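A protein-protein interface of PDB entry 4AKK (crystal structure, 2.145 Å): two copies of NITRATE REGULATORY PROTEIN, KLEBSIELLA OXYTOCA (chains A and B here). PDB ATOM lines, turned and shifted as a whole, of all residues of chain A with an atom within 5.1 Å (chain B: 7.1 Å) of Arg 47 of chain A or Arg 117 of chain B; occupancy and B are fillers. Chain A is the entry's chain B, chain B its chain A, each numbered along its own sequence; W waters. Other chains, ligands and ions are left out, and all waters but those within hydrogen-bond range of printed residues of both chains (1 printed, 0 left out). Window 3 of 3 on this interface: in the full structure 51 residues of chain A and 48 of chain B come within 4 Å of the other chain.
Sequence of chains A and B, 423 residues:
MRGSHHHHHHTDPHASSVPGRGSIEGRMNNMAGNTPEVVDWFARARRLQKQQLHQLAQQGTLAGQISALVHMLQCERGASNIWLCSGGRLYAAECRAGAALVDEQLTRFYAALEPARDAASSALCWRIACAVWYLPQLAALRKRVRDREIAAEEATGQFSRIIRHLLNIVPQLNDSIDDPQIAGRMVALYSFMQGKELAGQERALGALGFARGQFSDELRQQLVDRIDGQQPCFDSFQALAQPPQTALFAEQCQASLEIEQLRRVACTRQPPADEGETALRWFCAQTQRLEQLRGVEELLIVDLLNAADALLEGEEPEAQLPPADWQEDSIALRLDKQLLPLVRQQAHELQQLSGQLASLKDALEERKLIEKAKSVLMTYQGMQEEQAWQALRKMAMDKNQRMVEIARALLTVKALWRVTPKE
The backbone carbonyl oxygen (O) of Asp 118 of chain B is in hydrogen-bond range of the guanidinium group (NH2) of Arg 44 of chain A (3.4 Å).
The guanidinium group (NE) of Arg 44 of chain A sits at hydrogen-bond distance from the backbone carbonyl oxygen (O) of Arg 117 of chain B (2.9 Å).
The backbone carbonyl oxygen (O) of Ala 120 of chain B sits at hydrogen-bond distance from the guanidinium group (NE) of Arg 44 of chain A, 3.2 Å away.
OG of Ser 122 of chain B is in hydrogen-bond range of O of Ala 45 of chain A (3.5 Å).
OD1 of Asp 118 of chain B lies within salt-bridge range of NH1 of Arg 117 of chain B (3.9 Å).
SG of Cys 125 of chain B sits at hydrogen-bond distance from O of Ser 121 of chain B, at 3.3 Å.
The side-chain hydroxyl (OG) of Ser 121 of chain B lies within hydrogen-bond range of the backbone NH (N) of Leu 124 of chain B, at 3.2 Å.
Among the printed residues, merely in contact across the chains: Trp 41 of chain A with Leu 113 of chain B (3.9 Å), Trp 41 of chain A with Arg 117 of chain B (3.5 Å), Trp 41 of chain A with Ala 120 of chain B (3.9 Å), Trp 41 of chain A with Cys 125 of chain B (3.5 Å), Trp 41 of chain A with Ile 128 of chain B (3.4 Å), Arg 44 of chain A with Cys 125 of chain B (3.8 Å), Ala 45 of chain A with Cys 125 of chain B (3.6 Å), Arg 47 of chain A with Arg 117 of chain B (3.5 Å), Leu 48 of chain A with Ala 120 of chain B (3.1 Å), Leu 48 of chain A with Ser 121 of chain B (3.6 Å) and Leu 48 of chain A with Ser 122 of chain B (3.3 Å).
Asp 40 of chain A touches none of the printed residues of chain B.
Of the printed residues of chain B, Trp 41 of chain A touches Leu 113, Arg 117, Ala 120, Cys 125 and Ile 128.
Ala 43 of chain A touches none of the printed residues of chain B.
Printed residues of chain B within 4 Å of Arg 44 of chain A: Arg 117 (2.9 Å), Asp 118 (3.4 Å), Ala 120 (3.2 Å) and Cys 125 (3.8 Å).
Of chain A, only Trp 41, Arg 44 and Arg 47 come within 4 Å of Arg 117 of chain B.
The nearest printed residue of chain B that does not touch Arg 44 of chain A is Ala 119 of chain B (4.1 Å).
Of the 12 printed residues of chain A, 5 touch a printed residue of chain B.
Hydrophobic or aromatic side chains of chain B within 4 Å of the printed part of chain A: Ala 120 and Ile 128.
Among the printed residues, no Asp or Glu carboxylate lies within 4 Å of a Lys or Arg side-chain nitrogen of the other chain.
No position is printed for both chains.
Of the 15 pairs that touch across the chains among the printed residues, none has its exchanged pair printed and touching as well.
Water W1 lies within hydrogen-bond range of OE1 of Gln 49 of chain A (2.5 Å), OG of Ser 122 of chain B (2.9 Å) and O of Ala 45 of chain A (3.1 Å).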
ATOM      1  N   ASP A  40      -6.090  15.027   6.621  1.00  0.00           N
ATOM      2  CA  ASP A  40      -4.821  15.554   6.144  1.00  0.00           C
ATOM      3  C   ASP A  40      -3.965  14.489   5.460  1.00  0.00           C
ATOM      4  O   ASP A  40      -3.334  14.771   4.445  1.00  0.00           O
ATOM      5  CB  ASP A  40      -4.053  16.255   7.273  1.00  0.00           C
ATOM      6  CG  ASP A  40      -4.607  17.645   7.581  1.00  0.00           C
ATOM      7  OD1 ASP A  40      -5.643  18.027   6.986  1.00  0.00           O
ATOM      8  OD2 ASP A  40      -4.006  18.361   8.412  1.00  0.00           O
ATOM      9  N   TRP A  41      -3.954  13.272   5.997  1.00  0.00           N
ATOM     10  CA  TRP A  41      -3.199  12.195   5.362  1.00  0.00           C
ATOM     11  C   TRP A  41      -3.779  11.837   4.001  1.00  0.00           C
ATOM     12  O   TRP A  41      -3.042  11.514   3.081  1.00  0.00           O
ATOM     13  CB  TRP A  41      -3.091  10.968   6.267  1.00  0.00           C
ATOM     14  CG  TRP A  41      -2.107  11.164   7.372  1.00  0.00           C
ATOM     15  CD1 TRP A  41      -2.385  11.422   8.686  1.00  0.00           C
ATOM     16  CD2 TRP A  41      -0.678  11.149   7.261  1.00  0.00           C
ATOM     17  NE1 TRP A  41      -1.217  11.551   9.401  1.00  0.00           N
ATOM     18  CE2 TRP A  41      -0.156  11.388   8.548  1.00  0.00           C
ATOM     19  CE3 TRP A  41       0.210  10.942   6.201  1.00  0.00           C
ATOM     20  CZ2 TRP A  41       1.214  11.433   8.801  1.00  0.00           C
ATOM     21  CZ3 TRP A  41       1.568  10.988   6.452  1.00  0.00           C
ATOM     22  CH2 TRP A  41       2.057  11.230   7.743  1.00  0.00           C
ATOM     23  N   PHE A  42      -5.098  11.927   3.868  1.00  0.00           N
ATOM     24  CA  PHE A  42      -5.745  11.709   2.581  1.00  0.00           C
ATOM     25  C   PHE A  42      -5.490  12.856   1.633  1.00  0.00           C
ATOM     26  O   PHE A  42      -5.313  12.643   0.436  1.00  0.00           O
ATOM     27  CB  PHE A  42      -7.249  11.499   2.741  1.00  0.00           C
ATOM     28  CG  PHE A  42      -7.606  10.118   3.172  1.00  0.00           C
ATOM     29  CD1 PHE A  42      -7.384   9.044   2.326  1.00  0.00           C
ATOM     30  CD2 PHE A  42      -8.124   9.883   4.430  1.00  0.00           C
ATOM     31  CE1 PHE A  42      -7.689   7.760   2.721  1.00  0.00           C
ATOM     32  CE2 PHE A  42      -8.441   8.597   4.832  1.00  0.00           C
ATOM     33  CZ  PHE A  42      -8.222   7.534   3.975  1.00  0.00           C
ATOM     34  N   ALA A  43      -5.478  14.073   2.170  1.00  0.00           N
ATOM     35  CA  ALA A  43      -5.194  15.254   1.360  1.00  0.00           C
ATOM     36  C   ALA A  43      -3.816  15.149   0.729  1.00  0.00           C
ATOM     37  O   ALA A  43      -3.643  15.469  -0.448  1.00  0.00           O
ATOM     38  CB  ALA A  43      -5.297  16.519   2.194  1.00  0.00           C
ATOM     39  N   ARG A  44      -2.832  14.711   1.508  1.00  0.00           N
ATOM     40  CA  ARG A  44      -1.485  14.551   0.969  1.00  0.00           C
ATOM     41  C   ARG A  44      -1.439  13.394  -0.027  1.00  0.00           C
ATOM     42  O   ARG A  44      -0.915  13.543  -1.136  1.00  0.00           O
ATOM     43  CB  ARG A  44      -0.438  14.365   2.072  1.00  0.00           C
ATOM     44  CG  ARG A  44       0.984  14.191   1.500  1.00  0.00           C
ATOM     45  CD  ARG A  44       2.055  14.094   2.581  1.00  0.00           C
ATOM     46  NE  ARG A  44       3.359  13.701   2.030  1.00  0.00           N
ATOM     47  CZ  ARG A  44       4.225  14.536   1.453  1.00  0.00           C
ATOM     48  NH1 ARG A  44       3.940  15.824   1.335  1.00  0.00           N
ATOM     49  NH2 ARG A  44       5.382  14.084   0.989  1.00  0.00           N
ATOM     50  N   ALA A  45      -2.008  12.254   0.356  1.00  0.00           N
ATOM     51  CA  ALA A  45      -2.047  11.107  -0.545  1.00  0.00           C
ATOM     52  C   ALA A  45      -2.638  11.542  -1.881  1.00  0.00           C
ATOM     53  O   ALA A  45      -2.068  11.282  -2.942  1.00  0.00           O
ATOM     54  CB  ALA A  45      -2.840   9.966   0.072  1.00  0.00           C
ATOM     55  N   ARG A  46      -3.755  12.260  -1.820  1.00  0.00           N
ATOM     56  CA  ARG A  46      -4.415  12.753  -3.023  1.00  0.00           C
ATOM     57  C   ARG A  46      -3.600  13.798  -3.796  1.00  0.00           C
ATOM     58  O   ARG A  46      -3.606  13.802  -5.028  1.00  0.00           O
ATOM     59  CB  ARG A  46      -5.808  13.296  -2.685  1.00  0.00           C
ATOM     60  CG  ARG A  46      -6.810  12.208  -2.297  1.00  0.00           C
ATOM     61  CD  ARG A  46      -8.221  12.768  -2.105  1.00  0.00           C
ATOM     62  NE  ARG A  46      -8.380  13.477  -0.832  1.00  0.00           N
ATOM     63  CZ  ARG A  46      -8.414  14.802  -0.705  1.00  0.00           C
ATOM     64  NH1 ARG A  46      -8.305  15.583  -1.775  1.00  0.00           N
ATOM     65  NH2 ARG A  46      -8.560  15.350   0.495  1.00  0.00           N
ATOM     66  N   ARG A  47      -2.916  14.690  -3.083  1.00  0.00           N
ATOM     67  CA  ARG A  47      -2.025  15.654  -3.734  1.00  0.00           C
ATOM     68  C   ARG A  47      -0.919  14.936  -4.501  1.00  0.00           C
ATOM     69  O   ARG A  47      -0.648  15.250  -5.656  1.00  0.00           O
ATOM     70  CB  ARG A  47      -1.393  16.612  -2.716  1.00  0.00           C
ATOM     71  CG  ARG A  47      -2.301  17.749  -2.264  1.00  0.00           C
ATOM     72  CD  ARG A  47      -1.502  18.872  -1.610  1.00  0.00           C
ATOM     73  NE  ARG A  47      -0.791  18.429  -0.414  1.00  0.00           N
ATOM     74  CZ  ARG A  47      -1.337  18.350   0.795  1.00  0.00           C
ATOM     75  NH1 ARG A  47      -2.615  18.670   0.973  1.00  0.00           N
ATOM     76  NH2 ARG A  47      -0.607  17.940   1.826  1.00  0.00           N
ATOM     77  N   LEU A  48      -0.276  13.978  -3.837  1.00  0.00           N
ATOM     78  CA  LEU A  48       0.807  13.220  -4.448  1.00  0.00           C
ATOM     79  C   LEU A  48       0.322  12.516  -5.705  1.00  0.00           C
ATOM     80  O   LEU A  48       0.983  12.556  -6.741  1.00  0.00           O
ATOM     81  CB  LEU A  48       1.368  12.196  -3.468  1.00  0.00           C
ATOM     82  CG  LEU A  48       2.192  12.768  -2.315  1.00  0.00           C
ATOM     83  CD1 LEU A  48       2.527  11.680  -1.312  1.00  0.00           C
ATOM     84  CD2 LEU A  48       3.448  13.416  -2.856  1.00  0.00           C
ATOM     85  N   GLN A  49      -0.843  11.885  -5.615  1.00  0.00           N
ATOM     86  CA  GLN A  49      -1.345  11.117  -6.733  1.00  0.00           C
ATOM     87  C   GLN A  49      -1.653  12.008  -7.931  1.00  0.00           C
ATOM     88  O   GLN A  49      -1.379  11.630  -9.069  1.00  0.00           O
ATOM     89  CB  GLN A  49      -2.558  10.278  -6.334  1.00  0.00           C
ATOM     90  CG  GLN A  49      -3.143   9.506  -7.506  1.00  0.00           C
ATOM     91  CD  GLN A  49      -4.064   8.385  -7.073  1.00  0.00           C
ATOM     92  OE1 GLN A  49      -3.987   7.908  -5.939  1.00  0.00           O
ATOM     93  NE2 GLN A  49      -4.939   7.951  -7.979  1.00  0.00           N
ATOM     94  N   LYS A  50      -2.203  13.195  -7.680  1.00  0.00           N
ATOM     95  CA  LYS A  50      -2.504  14.120  -8.772  1.00  0.00           C
ATOM     96  C   LYS A  50      -1.237  14.584  -9.481  1.00  0.00           C
ATOM     97  O   LYS A  50      -1.226  14.756 -10.702  1.00  0.00           O
ATOM     98  CB  LYS A  50      -3.320  15.324  -8.289  1.00  0.00           C
ATOM     99  CG  LYS A  50      -4.828  15.101  -8.306  1.00  0.00           C
ATOM    100  CD  LYS A  50      -5.582  16.353  -7.864  1.00  0.00           C
ATOM    101  CE  LYS A  50      -7.090  16.128  -7.858  1.00  0.00           C
ATOM    102  NZ  LYS A  50      -7.850  17.328  -7.389  1.00  0.00           N
ATOM    103  N   GLN A  51      -0.171  14.789  -8.720  1.00  0.00           N
ATOM    104  CA  GLN A  51       1.109  15.140  -9.314  1.00  0.00           C
ATOM    105  C   GLN A  51       1.594  14.004 -10.207  1.00  0.00           C
ATOM    106  O   GLN A  51       2.043  14.227 -11.335  1.00  0.00           O
ATOM    107  CB  GLN A  51       2.143  15.430  -8.229  1.00  0.00           C
ATOM    108  CG  GLN A  51       1.663  16.420  -7.185  1.00  0.00           C
ATOM    109  CD  GLN A  51       2.710  16.715  -6.128  1.00  0.00           C
ATOM    110  OE1 GLN A  51       3.844  16.015  -6.196  1.00  0.00           O
ATOM    111  NE2 GLN A  51       2.504  17.566  -5.258  1.00  0.00           N
ATOM    112  N   GLN B  58      13.815   9.647  11.586  1.00  0.00           N
ATOM    113  CA  GLN B  58      12.378   9.709  11.791  1.00  0.00           C
ATOM    114  C   GLN B  58      11.716   8.378  11.409  1.00  0.00           C
ATOM    115  O   GLN B  58      10.755   7.944  12.046  1.00  0.00           O
ATOM    116  CB  GLN B  58      11.759  10.903  11.039  1.00  0.00           C
ATOM    117  CG  GLN B  58      11.891  10.871   9.508  1.00  0.00           C
ATOM    118  CD  GLN B  58      10.672  10.280   8.807  1.00  0.00           C
ATOM    119  OE1 GLN B  58       9.769   9.752   9.454  1.00  0.00           O
ATOM    120  NE2 GLN B  58      10.645  10.370   7.476  1.00  0.00           N
ATOM    121  N   ALA B 112       5.602  11.180  16.564  1.00  0.00           N
ATOM    122  CA  ALA B 112       6.505  10.599  15.574  1.00  0.00           C
ATOM    123  C   ALA B 112       5.947  10.694  14.150  1.00  0.00           C
ATOM    124  O   ALA B 112       6.698  10.578  13.182  1.00  0.00           O
ATOM    125  CB  ALA B 112       6.841   9.158  15.925  1.00  0.00           C
ATOM    126  N   LEU B 113       4.642  10.927  14.015  1.00  0.00           N
ATOM    127  CA  LEU B 113       4.051  11.077  12.675  1.00  0.00           C
ATOM    128  C   LEU B 113       4.359  12.428  12.000  1.00  0.00           C
ATOM    129  O   LEU B 113       4.371  12.517  10.770  1.00  0.00           O
ATOM    130  CB  LEU B 113       2.535  10.839  12.695  1.00  0.00           C
ATOM    131  CG  LEU B 113       2.028   9.405  12.884  1.00  0.00           C
ATOM    132  CD1 LEU B 113       0.513   9.390  12.886  1.00  0.00           C
ATOM    133  CD2 LEU B 113       2.565   8.489  11.802  1.00  0.00           C
ATOM    134  N   GLU B 114       4.605  13.469  12.797  1.00  0.00           N
ATOM    135  CA  GLU B 114       4.806  14.823  12.260  1.00  0.00           C
ATOM    136  C   GLU B 114       5.945  14.883  11.243  1.00  0.00           C
ATOM    137  O   GLU B 114       5.758  15.355  10.126  1.00  0.00           O
ATOM    138  CB  GLU B 114       5.027  15.845  13.396  1.00  0.00           C
ATOM    139  CG  GLU B 114       4.895  17.325  12.980  1.00  0.00           C
ATOM    140  CD  GLU B 114       6.205  17.949  12.480  1.00  0.00           C
ATOM    141  OE1 GLU B 114       7.255  17.761  13.138  1.00  0.00           O
ATOM    142  OE2 GLU B 114       6.182  18.649  11.438  1.00  0.00           O
ATOM    143  N   PRO B 115       7.135  14.399  11.628  1.00  0.00           N
ATOM    144  CA  PRO B 115       8.251  14.387  10.685  1.00  0.00           C
ATOM    145  C   PRO B 115       7.989  13.463   9.493  1.00  0.00           C
ATOM    146  O   PRO B 115       8.464  13.754   8.394  1.00  0.00           O
ATOM    147  CB  PRO B 115       9.418  13.867  11.535  1.00  0.00           C
ATOM    148  CG  PRO B 115       9.026  14.152  12.932  1.00  0.00           C
ATOM    149  CD  PRO B 115       7.552  13.970  12.974  1.00  0.00           C
ATOM    150  N   ALA B 116       7.236  12.383   9.694  1.00  0.00           N
ATOM    151  CA  ALA B 116       6.989  11.430   8.605  1.00  0.00           C
ATOM    152  C   ALA B 116       6.210  12.070   7.467  1.00  0.00           C
ATOM    153  O   ALA B 116       6.407  11.730   6.302  1.00  0.00           O
ATOM    154  CB  ALA B 116       6.264  10.184   9.113  1.00  0.00           C
ATOM    155  N   ARG B 117       5.324  12.995   7.824  1.00  0.00           N
ATOM    156  CA  ARG B 117       4.493  13.723   6.864  1.00  0.00           C
ATOM    157  C   ARG B 117       5.252  14.261   5.660  1.00  0.00           C
ATOM    158  O   ARG B 117       4.802  14.136   4.529  1.00  0.00           O
ATOM    159  CB  ARG B 117       3.832  14.914   7.554  1.00  0.00           C
ATOM    160  CG  ARG B 117       2.599  14.590   8.354  1.00  0.00           C
ATOM    161  CD  ARG B 117       1.553  15.686   8.155  1.00  0.00           C
ATOM    162  NE  ARG B 117       1.036  15.716   6.783  1.00  0.00           N
ATOM    163  CZ  ARG B 117       1.549  16.449   5.798  1.00  0.00           C
ATOM    164  NH1 ARG B 117       2.607  17.223   6.015  1.00  0.00           N
ATOM    165  NH2 ARG B 117       1.005  16.407   4.592  1.00  0.00           N
ATOM    166  N   ASP B 118       6.399  14.877   5.914  1.00  0.00           N
ATOM    167  CA  ASP B 118       7.139  15.579   4.877  1.00  0.00           C
ATOM    168  C   ASP B 118       7.755  14.641   3.844  1.00  0.00           C
ATOM    169  O   ASP B 118       8.072  15.060   2.733  1.00  0.00           O
ATOM    170  CB  ASP B 118       8.240  16.448   5.502  1.00  0.00           C
ATOM    171  CG  ASP B 118       7.685  17.585   6.349  1.00  0.00           C
ATOM    172  OD1 ASP B 118       6.483  17.922   6.208  1.00  0.00           O
ATOM    173  OD2 ASP B 118       8.460  18.146   7.154  1.00  0.00           O
ATOM    174  N   ALA B 119       7.928  13.375   4.206  1.00  0.00           N
ATOM    175  CA  ALA B 119       8.616  12.434   3.325  1.00  0.00           C
ATOM    176  C   ALA B 119       7.742  11.252   2.887  1.00  0.00           C
ATOM    177  O   ALA B 119       8.237  10.299   2.294  1.00  0.00           O
ATOM    178  CB  ALA B 119       9.882  11.927   3.998  1.00  0.00           C
ATOM    179  N   ALA B 120       6.451  11.315   3.183  1.00  0.00           N
ATOM    180  CA  ALA B 120       5.582  10.156   3.000  1.00  0.00           C
ATOM    181  C   ALA B 120       5.062   9.985   1.573  1.00  0.00           C
ATOM    182  O   ALA B 120       4.435  10.886   1.018  1.00  0.00           O
ATOM    183  CB  ALA B 120       4.423  10.227   3.971  1.00  0.00           C
ATOM    184  N   SER B 121       5.323   8.820   0.988  1.00  0.00           N
ATOM    185  CA  SER B 121       4.729   8.454  -0.291  1.00  0.00           C
ATOM    186  C   SER B 121       3.218   8.348  -0.145  1.00  0.00           C
ATOM    187  O   SER B 121       2.694   8.251   0.966  1.00  0.00           O
ATOM    188  CB  SER B 121       5.258   7.102  -0.750  1.00  0.00           C
ATOM    189  OG  SER B 121       4.770   6.080   0.104  1.00  0.00           O
ATOM    190  N   SER B 122       2.525   8.356  -1.277  1.00  0.00           N
ATOM    191  CA  SER B 122       1.081   8.207  -1.298  1.00  0.00           C
ATOM    192  C   SER B 122       0.634   6.930  -0.581  1.00  0.00           C
ATOM    193  O   SER B 122      -0.310   6.949   0.198  1.00  0.00           O
ATOM    194  CB  SER B 122       0.570   8.218  -2.744  1.00  0.00           C
ATOM    195  OG  SER B 122      -0.839   8.057  -2.778  1.00  0.00           O
ATOM    196  N   LEU B 124       2.219   5.251   1.790  1.00  0.00           N
ATOM    197  CA  LEU B 124       2.453   5.393   3.233  1.00  0.00           C
ATOM    198  C   LEU B 124       1.368   6.244   3.882  1.00  0.00           C
ATOM    199  O   LEU B 124       0.875   5.935   4.970  1.00  0.00           O
ATOM    200  CB  LEU B 124       3.839   5.984   3.523  1.00  0.00           C
ATOM    201  CG  LEU B 124       4.209   6.028   5.008  1.00  0.00           C
ATOM    202  CD1 LEU B 124       4.270   4.610   5.588  1.00  0.00           C
ATOM    203  CD2 LEU B 124       5.538   6.761   5.213  1.00  0.00           C
ATOM    204  N   CYS B 125       0.989   7.319   3.206  1.00  0.00           N
ATOM    205  CA  CYS B 125      -0.142   8.123   3.654  1.00  0.00           C
ATOM    206  C   CYS B 125      -1.403   7.291   3.850  1.00  0.00           C
ATOM    207  O   CYS B 125      -2.115   7.452   4.854  1.00  0.00           O
ATOM    208  CB  CYS B 125      -0.424   9.252   2.671  1.00  0.00           C
ATOM    209  SG  CYS B 125       0.903  10.477   2.569  1.00  0.00           S
ATOM    210  N   ILE B 128      -1.039   5.010   6.953  1.00  0.00           N
ATOM    211  CA  ILE B 128      -1.152   5.837   8.144  1.00  0.00           C
ATOM    212  C   ILE B 128      -2.597   6.304   8.375  1.00  0.00           C
ATOM    213  O   ILE B 128      -3.096   6.253   9.495  1.00  0.00           O
ATOM    214  CB  ILE B 128      -0.175   7.033   8.068  1.00  0.00           C
ATOM    215  CG1 ILE B 128       1.271   6.528   8.161  1.00  0.00           C
ATOM    216  CG2 ILE B 128      -0.456   8.041   9.182  1.00  0.00           C
ATOM    217  CD1 ILE B 128       2.298   7.518   7.675  1.00  0.00           C
HETATM  218  O   HOH W   1      -3.560   8.600  -3.525  1.00  0.00           O
